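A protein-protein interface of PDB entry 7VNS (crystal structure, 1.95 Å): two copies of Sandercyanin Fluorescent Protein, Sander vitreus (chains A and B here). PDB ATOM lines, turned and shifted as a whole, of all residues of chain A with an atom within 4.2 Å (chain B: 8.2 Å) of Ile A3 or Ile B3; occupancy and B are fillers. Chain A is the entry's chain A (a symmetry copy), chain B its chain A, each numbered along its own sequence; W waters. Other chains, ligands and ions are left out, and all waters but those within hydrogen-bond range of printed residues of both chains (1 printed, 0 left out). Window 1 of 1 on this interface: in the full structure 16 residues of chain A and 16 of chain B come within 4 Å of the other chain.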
ATOM      1  N   MET A   1       3.533 -18.897   1.589  1.00  0.00           N
ATOM      2  CA  MET A   1       3.304 -18.167   2.842  1.00  0.00           C
ATOM      3  C   MET A   1       2.728 -16.801   2.498  1.00  0.00           C
ATOM      4  O   MET A   1       3.009 -16.250   1.407  1.00  0.00           O
ATOM      5  CB  MET A   1       4.593 -17.994   3.633  1.00  0.00           C
ATOM      6  CG  MET A   1       5.134 -19.281   4.080  1.00  0.00           C
ATOM      7  SD  MET A   1       6.572 -19.125   5.094  1.00  0.00           S
ATOM      8  CE  MET A   1       5.901 -18.756   6.718  1.00  0.00           C
ATOM      9  N   PHE A   2       1.899 -16.304   3.396  1.00  0.00           N
ATOM     10  CA  PHE A   2       1.084 -15.075   3.209  1.00  0.00           C
ATOM     11  C   PHE A   2       1.890 -13.858   3.731  1.00  0.00           C
ATOM     12  O   PHE A   2       2.118 -13.867   4.982  1.00  0.00           O
ATOM     13  CB  PHE A   2      -0.253 -15.294   3.933  1.00  0.00           C
ATOM     14  CG  PHE A   2      -1.306 -14.238   3.716  1.00  0.00           C
ATOM     15  CD1 PHE A   2      -1.953 -14.114   2.489  1.00  0.00           C
ATOM     16  CD2 PHE A   2      -1.678 -13.383   4.747  1.00  0.00           C
ATOM     17  CE1 PHE A   2      -2.944 -13.156   2.294  1.00  0.00           C
ATOM     18  CE2 PHE A   2      -2.676 -12.436   4.550  1.00  0.00           C
ATOM     19  CZ  PHE A   2      -3.302 -12.319   3.325  1.00  0.00           C
ATOM     20  N   ILE A   3       2.249 -12.914   2.836  1.00  0.00           N
ATOM     21  CA  ILE A   3       3.080 -11.688   3.093  1.00  0.00           C
ATOM     22  C   ILE A   3       2.220 -10.495   3.467  1.00  0.00           C
ATOM     23  O   ILE A   3       1.394 -10.096   2.680  1.00  0.00           O
ATOM     24  CB  ILE A   3       3.985 -11.273   1.923  1.00  0.00           C
ATOM     25  CG1 ILE A   3       5.043 -12.344   1.671  1.00  0.00           C
ATOM     26  CG2 ILE A   3       4.687  -9.950   2.170  1.00  0.00           C
ATOM     27  CD1 ILE A   3       6.351 -11.772   1.140  1.00  0.00           C
ATOM     28  N   LYS A   4       2.562  -9.880   4.575  1.00  0.00           N
ATOM     29  CA  LYS A   4       1.794  -8.792   5.178  1.00  0.00           C
ATOM     30  C   LYS A   4       2.765  -7.825   5.838  1.00  0.00           C
ATOM     31  O   LYS A   4       3.893  -8.181   6.213  1.00  0.00           O
ATOM     32  CB  LYS A   4       0.837  -9.372   6.218  1.00  0.00           C
ATOM     33  CG  LYS A   4      -0.188 -10.337   5.642  1.00  0.00           C
ATOM     34  CD  LYS A   4      -1.155  -9.656   4.686  1.00  0.00           C
ATOM     35  CE  LYS A   4      -2.343  -9.022   5.381  1.00  0.00           C
ATOM     36  NZ  LYS A   4      -3.208  -8.297   4.417  1.00  0.00           N
ATOM     37  N   PHE A  36       1.550 -21.198  -2.824  1.00  0.00           N
ATOM     38  CA  PHE A  36       2.092 -22.482  -3.354  1.00  0.00           C
ATOM     39  C   PHE A  36       1.404 -23.687  -2.673  1.00  0.00           C
ATOM     40  O   PHE A  36       1.889 -24.818  -2.790  1.00  0.00           O
ATOM     41  CB  PHE A  36       3.620 -22.482  -3.254  1.00  0.00           C
ATOM     42  CG  PHE A  36       4.279 -21.302  -3.937  1.00  0.00           C
ATOM     43  CD1 PHE A  36       4.152 -21.110  -5.306  1.00  0.00           C
ATOM     44  CD2 PHE A  36       4.974 -20.347  -3.202  1.00  0.00           C
ATOM     45  CE1 PHE A  36       4.737 -20.012  -5.926  1.00  0.00           C
ATOM     46  CE2 PHE A  36       5.556 -19.249  -3.822  1.00  0.00           C
ATOM     47  CZ  PHE A  36       5.433 -19.081  -5.181  1.00  0.00           C
ATOM     48  N   LEU A 116      10.512 -10.417   7.368  1.00  0.00           N
ATOM     49  CA  LEU A 116      10.999  -9.937   6.063  1.00  0.00           C
ATOM     50  C   LEU A 116      11.218  -8.428   6.243  1.00  0.00           C
ATOM     51  O   LEU A 116      10.422  -7.603   5.704  1.00  0.00           O
ATOM     52  CB  LEU A 116       9.944 -10.228   4.986  1.00  0.00           C
ATOM     53  CG  LEU A 116       9.612 -11.695   4.717  1.00  0.00           C
ATOM     54  CD1 LEU A 116       8.509 -11.791   3.708  1.00  0.00           C
ATOM     55  CD2 LEU A 116      10.854 -12.499   4.269  1.00  0.00           C
ATOM     56  N   HIS A 120       6.334  -9.411   6.942  1.00  0.00           N
ATOM     57  CA  HIS A 120       6.475 -10.823   7.398  1.00  0.00           C
ATOM     58  C   HIS A 120       5.683 -11.738   6.500  1.00  0.00           C
ATOM     59  O   HIS A 120       4.824 -11.251   5.717  1.00  0.00           O
ATOM     60  CB  HIS A 120       6.134 -10.941   8.880  1.00  0.00           C
ATOM     61  CG  HIS A 120       4.662 -10.904   9.115  1.00  0.00           C
ATOM     62  ND1 HIS A 120       3.991  -9.708   9.258  1.00  0.00           N
ATOM     63  CD2 HIS A 120       3.721 -11.876   9.070  1.00  0.00           C
ATOM     64  CE1 HIS A 120       2.688  -9.972   9.421  1.00  0.00           C
ATOM     65  NE2 HIS A 120       2.486 -11.270   9.221  1.00  0.00           N
ATOM     66  N   ALA A 121       5.998 -13.028   6.573  1.00  0.00           N
ATOM     67  CA  ALA A 121       5.240 -14.089   5.906  1.00  0.00           C
ATOM     68  C   ALA A 121       4.774 -15.065   6.982  1.00  0.00           C
ATOM     69  O   ALA A 121       5.583 -15.382   7.865  1.00  0.00           O
ATOM     70  CB  ALA A 121       6.112 -14.772   4.896  1.00  0.00           C
ATOM     71  N   MET B   1       9.086  -7.342  -0.221  1.00  0.00           N
ATOM     72  CA  MET B   1      10.017  -8.307  -0.818  1.00  0.00           C
ATOM     73  C   MET B   1       9.227  -9.217  -1.748  1.00  0.00           C
ATOM     74  O   MET B   1       8.016  -9.457  -1.525  1.00  0.00           O
ATOM     75  CB  MET B   1      10.714  -9.144   0.244  1.00  0.00           C
ATOM     76  CG  MET B   1      11.574  -8.325   1.105  1.00  0.00           C
ATOM     77  SD  MET B   1      12.488  -9.267   2.286  1.00  0.00           S
ATOM     78  CE  MET B   1      13.886  -9.880   1.342  1.00  0.00           C
ATOM     79  N   PHE B   2       9.898  -9.661  -2.794  1.00  0.00           N
ATOM     80  CA  PHE B   2       9.301 -10.418  -3.926  1.00  0.00           C
ATOM     81  C   PHE B   2       9.388 -11.933  -3.613  1.00  0.00           C
ATOM     82  O   PHE B   2      10.571 -12.396  -3.547  1.00  0.00           O
ATOM     83  CB  PHE B   2      10.044 -10.000  -5.203  1.00  0.00           C
ATOM     84  CG  PHE B   2       9.475 -10.514  -6.500  1.00  0.00           C
ATOM     85  CD1 PHE B   2       8.273 -10.020  -6.999  1.00  0.00           C
ATOM     86  CD2 PHE B   2      10.154 -11.472  -7.245  1.00  0.00           C
ATOM     87  CE1 PHE B   2       7.757 -10.474  -8.211  1.00  0.00           C
ATOM     88  CE2 PHE B   2       9.641 -11.913  -8.458  1.00  0.00           C
ATOM     89  CZ  PHE B   2       8.443 -11.421  -8.935  1.00  0.00           C
ATOM     90  N   ILE B   3       8.231 -12.610  -3.464  1.00  0.00           N
ATOM     91  CA  ILE B   3       8.066 -14.059  -3.098  1.00  0.00           C
ATOM     92  C   ILE B   3       8.009 -14.945  -4.329  1.00  0.00           C
ATOM     93  O   ILE B   3       7.127 -14.773  -5.137  1.00  0.00           O
ATOM     94  CB  ILE B   3       6.833 -14.365  -2.235  1.00  0.00           C
ATOM     95  CG1 ILE B   3       6.965 -13.692  -0.871  1.00  0.00           C
ATOM     96  CG2 ILE B   3       6.626 -15.852  -2.021  1.00  0.00           C
ATOM     97  CD1 ILE B   3       6.284 -14.473   0.244  1.00  0.00           C
ATOM     98  N   LYS B   4       8.847 -15.955  -4.335  1.00  0.00           N
ATOM     99  CA  LYS B   4       9.042 -16.851  -5.474  1.00  0.00           C
ATOM    100  C   LYS B   4       9.346 -18.244  -4.944  1.00  0.00           C
ATOM    101  O   LYS B   4       9.828 -18.427  -3.815  1.00  0.00           O
ATOM    102  CB  LYS B   4      10.208 -16.341  -6.318  1.00  0.00           C
ATOM    103  CG  LYS B   4       9.983 -14.958  -6.910  1.00  0.00           C
ATOM    104  CD  LYS B   4       8.845 -14.935  -7.918  1.00  0.00           C
ATOM    105  CE  LYS B   4       9.276 -15.316  -9.321  1.00  0.00           C
ATOM    106  NZ  LYS B   4       8.115 -15.364 -10.246  1.00  0.00           N
ATOM    107  N   PRO B   5       9.110 -19.239  -5.798  1.00  0.00           N
ATOM    108  CA  PRO B   5       9.423 -20.614  -5.480  1.00  0.00           C
ATOM    109  C   PRO B   5      10.921 -20.836  -5.340  1.00  0.00           C
ATOM    110  O   PRO B   5      11.697 -20.155  -5.976  1.00  0.00           O
ATOM    111  CB  PRO B   5       8.944 -21.427  -6.691  1.00  0.00           C
ATOM    112  CG  PRO B   5       8.026 -20.496  -7.439  1.00  0.00           C
ATOM    113  CD  PRO B   5       8.462 -19.086  -7.124  1.00  0.00           C
ATOM    114  N   GLY B   6      11.247 -21.859  -4.566  1.00  0.00           N
ATOM    115  CA  GLY B   6      12.623 -22.301  -4.398  1.00  0.00           C
ATOM    116  C   GLY B   6      13.211 -21.652  -3.190  1.00  0.00           C
ATOM    117  O   GLY B   6      12.802 -20.563  -2.836  1.00  0.00           O
ATOM    118  N   LEU B  32      13.779  -5.575  -8.358  1.00  0.00           N
ATOM    119  CA  LEU B  32      12.607  -6.480  -8.282  1.00  0.00           C
ATOM    120  C   LEU B  32      11.418  -5.716  -7.761  1.00  0.00           C
ATOM    121  O   LEU B  32      11.549  -4.822  -6.946  1.00  0.00           O
ATOM    122  CB  LEU B  32      12.877  -7.658  -7.347  1.00  0.00           C
ATOM    123  CG  LEU B  32      13.819  -8.713  -7.891  1.00  0.00           C
ATOM    124  CD1 LEU B  32      14.084  -9.745  -6.767  1.00  0.00           C
ATOM    125  CD2 LEU B  32      13.204  -9.344  -9.149  1.00  0.00           C
ATOM    126  N   PRO B  33      10.197  -6.100  -8.187  1.00  0.00           N
ATOM    127  CA  PRO B  33       8.989  -5.555  -7.587  1.00  0.00           C
ATOM    128  C   PRO B  33       8.982  -5.802  -6.072  1.00  0.00           C
ATOM    129  O   PRO B  33       9.476  -6.796  -5.530  1.00  0.00           O
ATOM    130  CB  PRO B  33       7.806  -6.256  -8.303  1.00  0.00           C
ATOM    131  CG  PRO B  33       8.422  -6.924  -9.521  1.00  0.00           C
ATOM    132  CD  PRO B  33       9.906  -7.104  -9.217  1.00  0.00           C
ATOM    133  N   ASN B  34       8.386  -4.857  -5.389  1.00  0.00           N
ATOM    134  CA  ASN B  34       8.470  -4.752  -3.917  1.00  0.00           C
ATOM    135  C   ASN B  34       7.126  -4.163  -3.506  1.00  0.00           C
ATOM    136  O   ASN B  34       6.916  -2.958  -3.737  1.00  0.00           O
ATOM    137  CB  ASN B  34       9.767  -4.003  -3.576  1.00  0.00           C
ATOM    138  CG  ASN B  34       9.850  -3.602  -2.126  1.00  0.00           C
ATOM    139  OD1 ASN B  34       9.144  -4.199  -1.308  1.00  0.00           O
ATOM    140  ND2 ASN B  34      10.659  -2.582  -1.829  1.00  0.00           N
ATOM    141  N   LYS B  35       6.216  -5.017  -3.045  1.00  0.00           N
ATOM    142  CA  LYS B  35       4.822  -4.673  -2.673  1.00  0.00           C
ATOM    143  C   LYS B  35       4.730  -3.456  -1.724  1.00  0.00           C
ATOM    144  O   LYS B  35       3.720  -2.728  -1.785  1.00  0.00           O
ATOM    145  CB  LYS B  35       4.225  -5.922  -2.017  1.00  0.00           C
ATOM    146  CG  LYS B  35       2.714  -5.960  -1.882  1.00  0.00           C
ATOM    147  CD  LYS B  35       2.223  -7.362  -1.528  1.00  0.00           C
ATOM    148  CE  LYS B  35       1.068  -7.386  -0.546  1.00  0.00           C
ATOM    149  NZ  LYS B  35      -0.111  -6.669  -1.081  1.00  0.00           N
ATOM    150  N   PHE B  36       5.691  -3.243  -0.828  1.00  0.00           N
ATOM    151  CA  PHE B  36       5.629  -2.120   0.150  1.00  0.00           C
ATOM    152  C   PHE B  36       6.670  -1.033  -0.201  1.00  0.00           C
ATOM    153  O   PHE B  36       6.945  -0.156   0.627  1.00  0.00           O
ATOM    154  CB  PHE B  36       5.735  -2.667   1.577  1.00  0.00           C
ATOM    155  CG  PHE B  36       4.700  -3.721   1.908  1.00  0.00           C
ATOM    156  CD1 PHE B  36       3.345  -3.418   1.895  1.00  0.00           C
ATOM    157  CD2 PHE B  36       5.077  -5.033   2.173  1.00  0.00           C
ATOM    158  CE1 PHE B  36       2.397  -4.394   2.175  1.00  0.00           C
ATOM    159  CE2 PHE B  36       4.127  -6.009   2.451  1.00  0.00           C
ATOM    160  CZ  PHE B  36       2.791  -5.688   2.447  1.00  0.00           C
ATOM    161  N   ILE B 114      15.664 -14.153   1.813  1.00  0.00           N
ATOM    162  CA  ILE B 114      15.262 -14.813   3.072  1.00  0.00           C
ATOM    163  C   ILE B 114      14.416 -16.031   2.701  1.00  0.00           C
ATOM    164  O   ILE B 114      13.477 -15.908   1.915  1.00  0.00           O
ATOM    165  CB  ILE B 114      14.534 -13.826   3.996  1.00  0.00           C
ATOM    166  CG1 ILE B 114      15.443 -12.706   4.494  1.00  0.00           C
ATOM    167  CG2 ILE B 114      13.861 -14.541   5.164  1.00  0.00           C
ATOM    168  CD1 ILE B 114      14.674 -11.455   4.906  1.00  0.00           C
ATOM    169  N   LEU B 116      11.726 -19.038   2.980  1.00  0.00           N
ATOM    170  CA  LEU B 116      10.340 -19.218   3.446  1.00  0.00           C
ATOM    171  C   LEU B 116      10.002 -20.687   3.155  1.00  0.00           C
ATOM    172  O   LEU B 116       9.210 -20.981   2.212  1.00  0.00           O
ATOM    173  CB  LEU B 116       9.416 -18.265   2.674  1.00  0.00           C
ATOM    174  CG  LEU B 116       9.653 -16.766   2.857  1.00  0.00           C
ATOM    175  CD1 LEU B 116       8.727 -15.992   1.971  1.00  0.00           C
ATOM    176  CD2 LEU B 116       9.514 -16.331   4.333  1.00  0.00           C
ATOM    177  N   SER B 119      10.150 -21.916  -0.450  1.00  0.00           N
ATOM    178  CA  SER B 119      10.026 -20.653  -1.230  1.00  0.00           C
ATOM    179  C   SER B 119      10.923 -19.570  -0.626  1.00  0.00           C
ATOM    180  O   SER B 119      11.656 -19.862   0.360  1.00  0.00           O
ATOM    181  CB  SER B 119       8.611 -20.209  -1.217  1.00  0.00           C
ATOM    182  OG  SER B 119       7.834 -21.166  -1.901  1.00  0.00           O
ATOM    183  N   HIS B 120      10.950 -18.388  -1.218  1.00  0.00           N
ATOM    184  CA  HIS B 120      11.857 -17.326  -0.698  1.00  0.00           C
ATOM    185  C   HIS B 120      11.314 -15.965  -1.046  1.00  0.00           C
ATOM    186  O   HIS B 120      10.404 -15.861  -1.912  1.00  0.00           O
ATOM    187  CB  HIS B 120      13.289 -17.573  -1.160  1.00  0.00           C
ATOM    188  CG  HIS B 120      13.485 -17.184  -2.587  1.00  0.00           C
ATOM    189  ND1 HIS B 120      13.210 -18.064  -3.611  1.00  0.00           N
ATOM    190  CD2 HIS B 120      13.762 -15.990  -3.160  1.00  0.00           C
ATOM    191  CE1 HIS B 120      13.442 -17.441  -4.775  1.00  0.00           C
ATOM    192  NE2 HIS B 120      13.690 -16.158  -4.533  1.00  0.00           N
ATOM    193  N   ALA B 121      11.819 -14.949  -0.352  1.00  0.00           N
ATOM    194  CA  ALA B 121      11.543 -13.543  -0.651  1.00  0.00           C
ATOM    195  C   ALA B 121      12.881 -12.858  -0.912  1.00  0.00           C
ATOM    196  O   ALA B 121      13.826 -13.127  -0.158  1.00  0.00           O
ATOM    197  CB  ALA B 121      10.830 -12.912   0.507  1.00  0.00           C
ATOM    198  N   ALA B 122      12.953 -11.970  -1.897  1.00  0.00           N
ATOM    199  CA  ALA B 122      14.229 -11.329  -2.252  1.00  0.00           C
ATOM    200  C   ALA B 122      14.048  -9.845  -2.568  1.00  0.00           C
ATOM    201  O   ALA B 122      12.963  -9.410  -2.967  1.00  0.00           O
ATOM    202  CB  ALA B 122      14.869 -12.095  -3.369  1.00  0.00           C
ATOM    203  N   TYR B 123      15.095  -9.082  -2.337  1.00  0.00           N
ATOM    204  CA  TYR B 123      15.329  -7.769  -2.994  1.00  0.00           C
ATOM    205  C   TYR B 123      16.472  -7.984  -3.968  1.00  0.00           C
ATOM    206  O   TYR B 123      17.421  -8.776  -3.676  1.00  0.00           O
ATOM    207  CB  TYR B 123      15.835  -6.714  -2.015  1.00  0.00           C
ATOM    208  CG  TYR B 123      14.882  -6.248  -0.960  1.00  0.00           C
ATOM    209  CD1 TYR B 123      13.875  -5.356  -1.282  1.00  0.00           C
ATOM    210  CD2 TYR B 123      15.034  -6.607   0.361  1.00  0.00           C
ATOM    211  CE1 TYR B 123      13.002  -4.869  -0.318  1.00  0.00           C
ATOM    212  CE2 TYR B 123      14.181  -6.116   1.345  1.00  0.00           C
ATOM    213  CZ  TYR B 123      13.173  -5.231   1.007  1.00  0.00           C
ATOM    214  OH  TYR B 123      12.325  -4.724   1.961  1.00  0.00           O
HETATM  215  O   HOH W   1      11.173  -5.264   4.300  1.00  0.00           O
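Water W1 bridges the side-chain hydroxyl (OH) of Tyr B123 (2.7 Å) and the backbone carbonyl oxygen (O) of Leu A116 (2.8 Å).
Of the 18 printed residues of chain B, 8 touch a printed residue of chain A.
Hydrophobic or aromatic side chains of chain B within 4 Å of the printed part of chain A: Met B1, Ile B3, Pro B5, Phe B36, Ile B114, Leu B116 and Ala B121.
Hydrophobic or aromatic side chains of chain A that line the printed part of chain B: Met A1, Ile A3, Phe A36, Leu A116 and Ala A121.
Among the printed residues, 12 pairs touch across the chains.
Among the printed residues, no Asp or Glu carboxylate lies within 4 Å of a Lys or Arg side-chain nitrogen of the other chain.
Of the printed residues of chain A, Ile B3 touches Met A1, Ile A3 and Phe A36.
Of the printed residues of chain A, Ile B114 touches Leu A116.
Of the printed residues of chain A, Ser B119 touches Phe A36.
Of the printed residues of chain A, Met B1 touches Ile A3 (3.9 Å) and Leu A116 (3.8 Å).
The nearest printed residue of chain B that does not touch Ile A3 is Lys B35 (4.2 Å).
Met A1 touches Ile B3 (O to CD1, 3.9 Å).
Leu B116 touches Met A1.
Ile A3 touches Met B1.
Ile A3 touches Phe B36.
Ile B3 touches Phe A36 (CG2 to CE2, 3.99 Å).
Phe A36 touches Pro B5.
Phe A36 touches Ser B119.
Met B1 touches Leu A116 (SD to CB, 3.8 Å).
CD2 of Leu A116 touches CG2 of Ile B114, at 3.7 Å.
Leu B116 touches Ala A121 (CD2 to CB, 3.8 Å).
The side-chain amide oxygen of Asn B34 sits at hydrogen-bond distance from the backbone NH of Met B1, at 3.3 Å.
The backbone carbonyl oxygen (O) of Ala B121 sits at hydrogen-bond distance from the backbone NH (N) of Ile B114.
Met A1 touches Ile B3, and with the chains exchanged Ile A3 touches Met B1.
Met A1 touches Leu B116, and with the chains exchanged Leu A116 touches Met B1.
Ile A3 touches Phe B36, and with the chains exchanged Phe A36 touches Ile B3.
Leu A116 touches Ala B121, and with the chains exchanged Ala A121 touches Leu B116.
Positions printed for both chains: 1, 2, 3, 4, 36, 116, 120 and 121.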
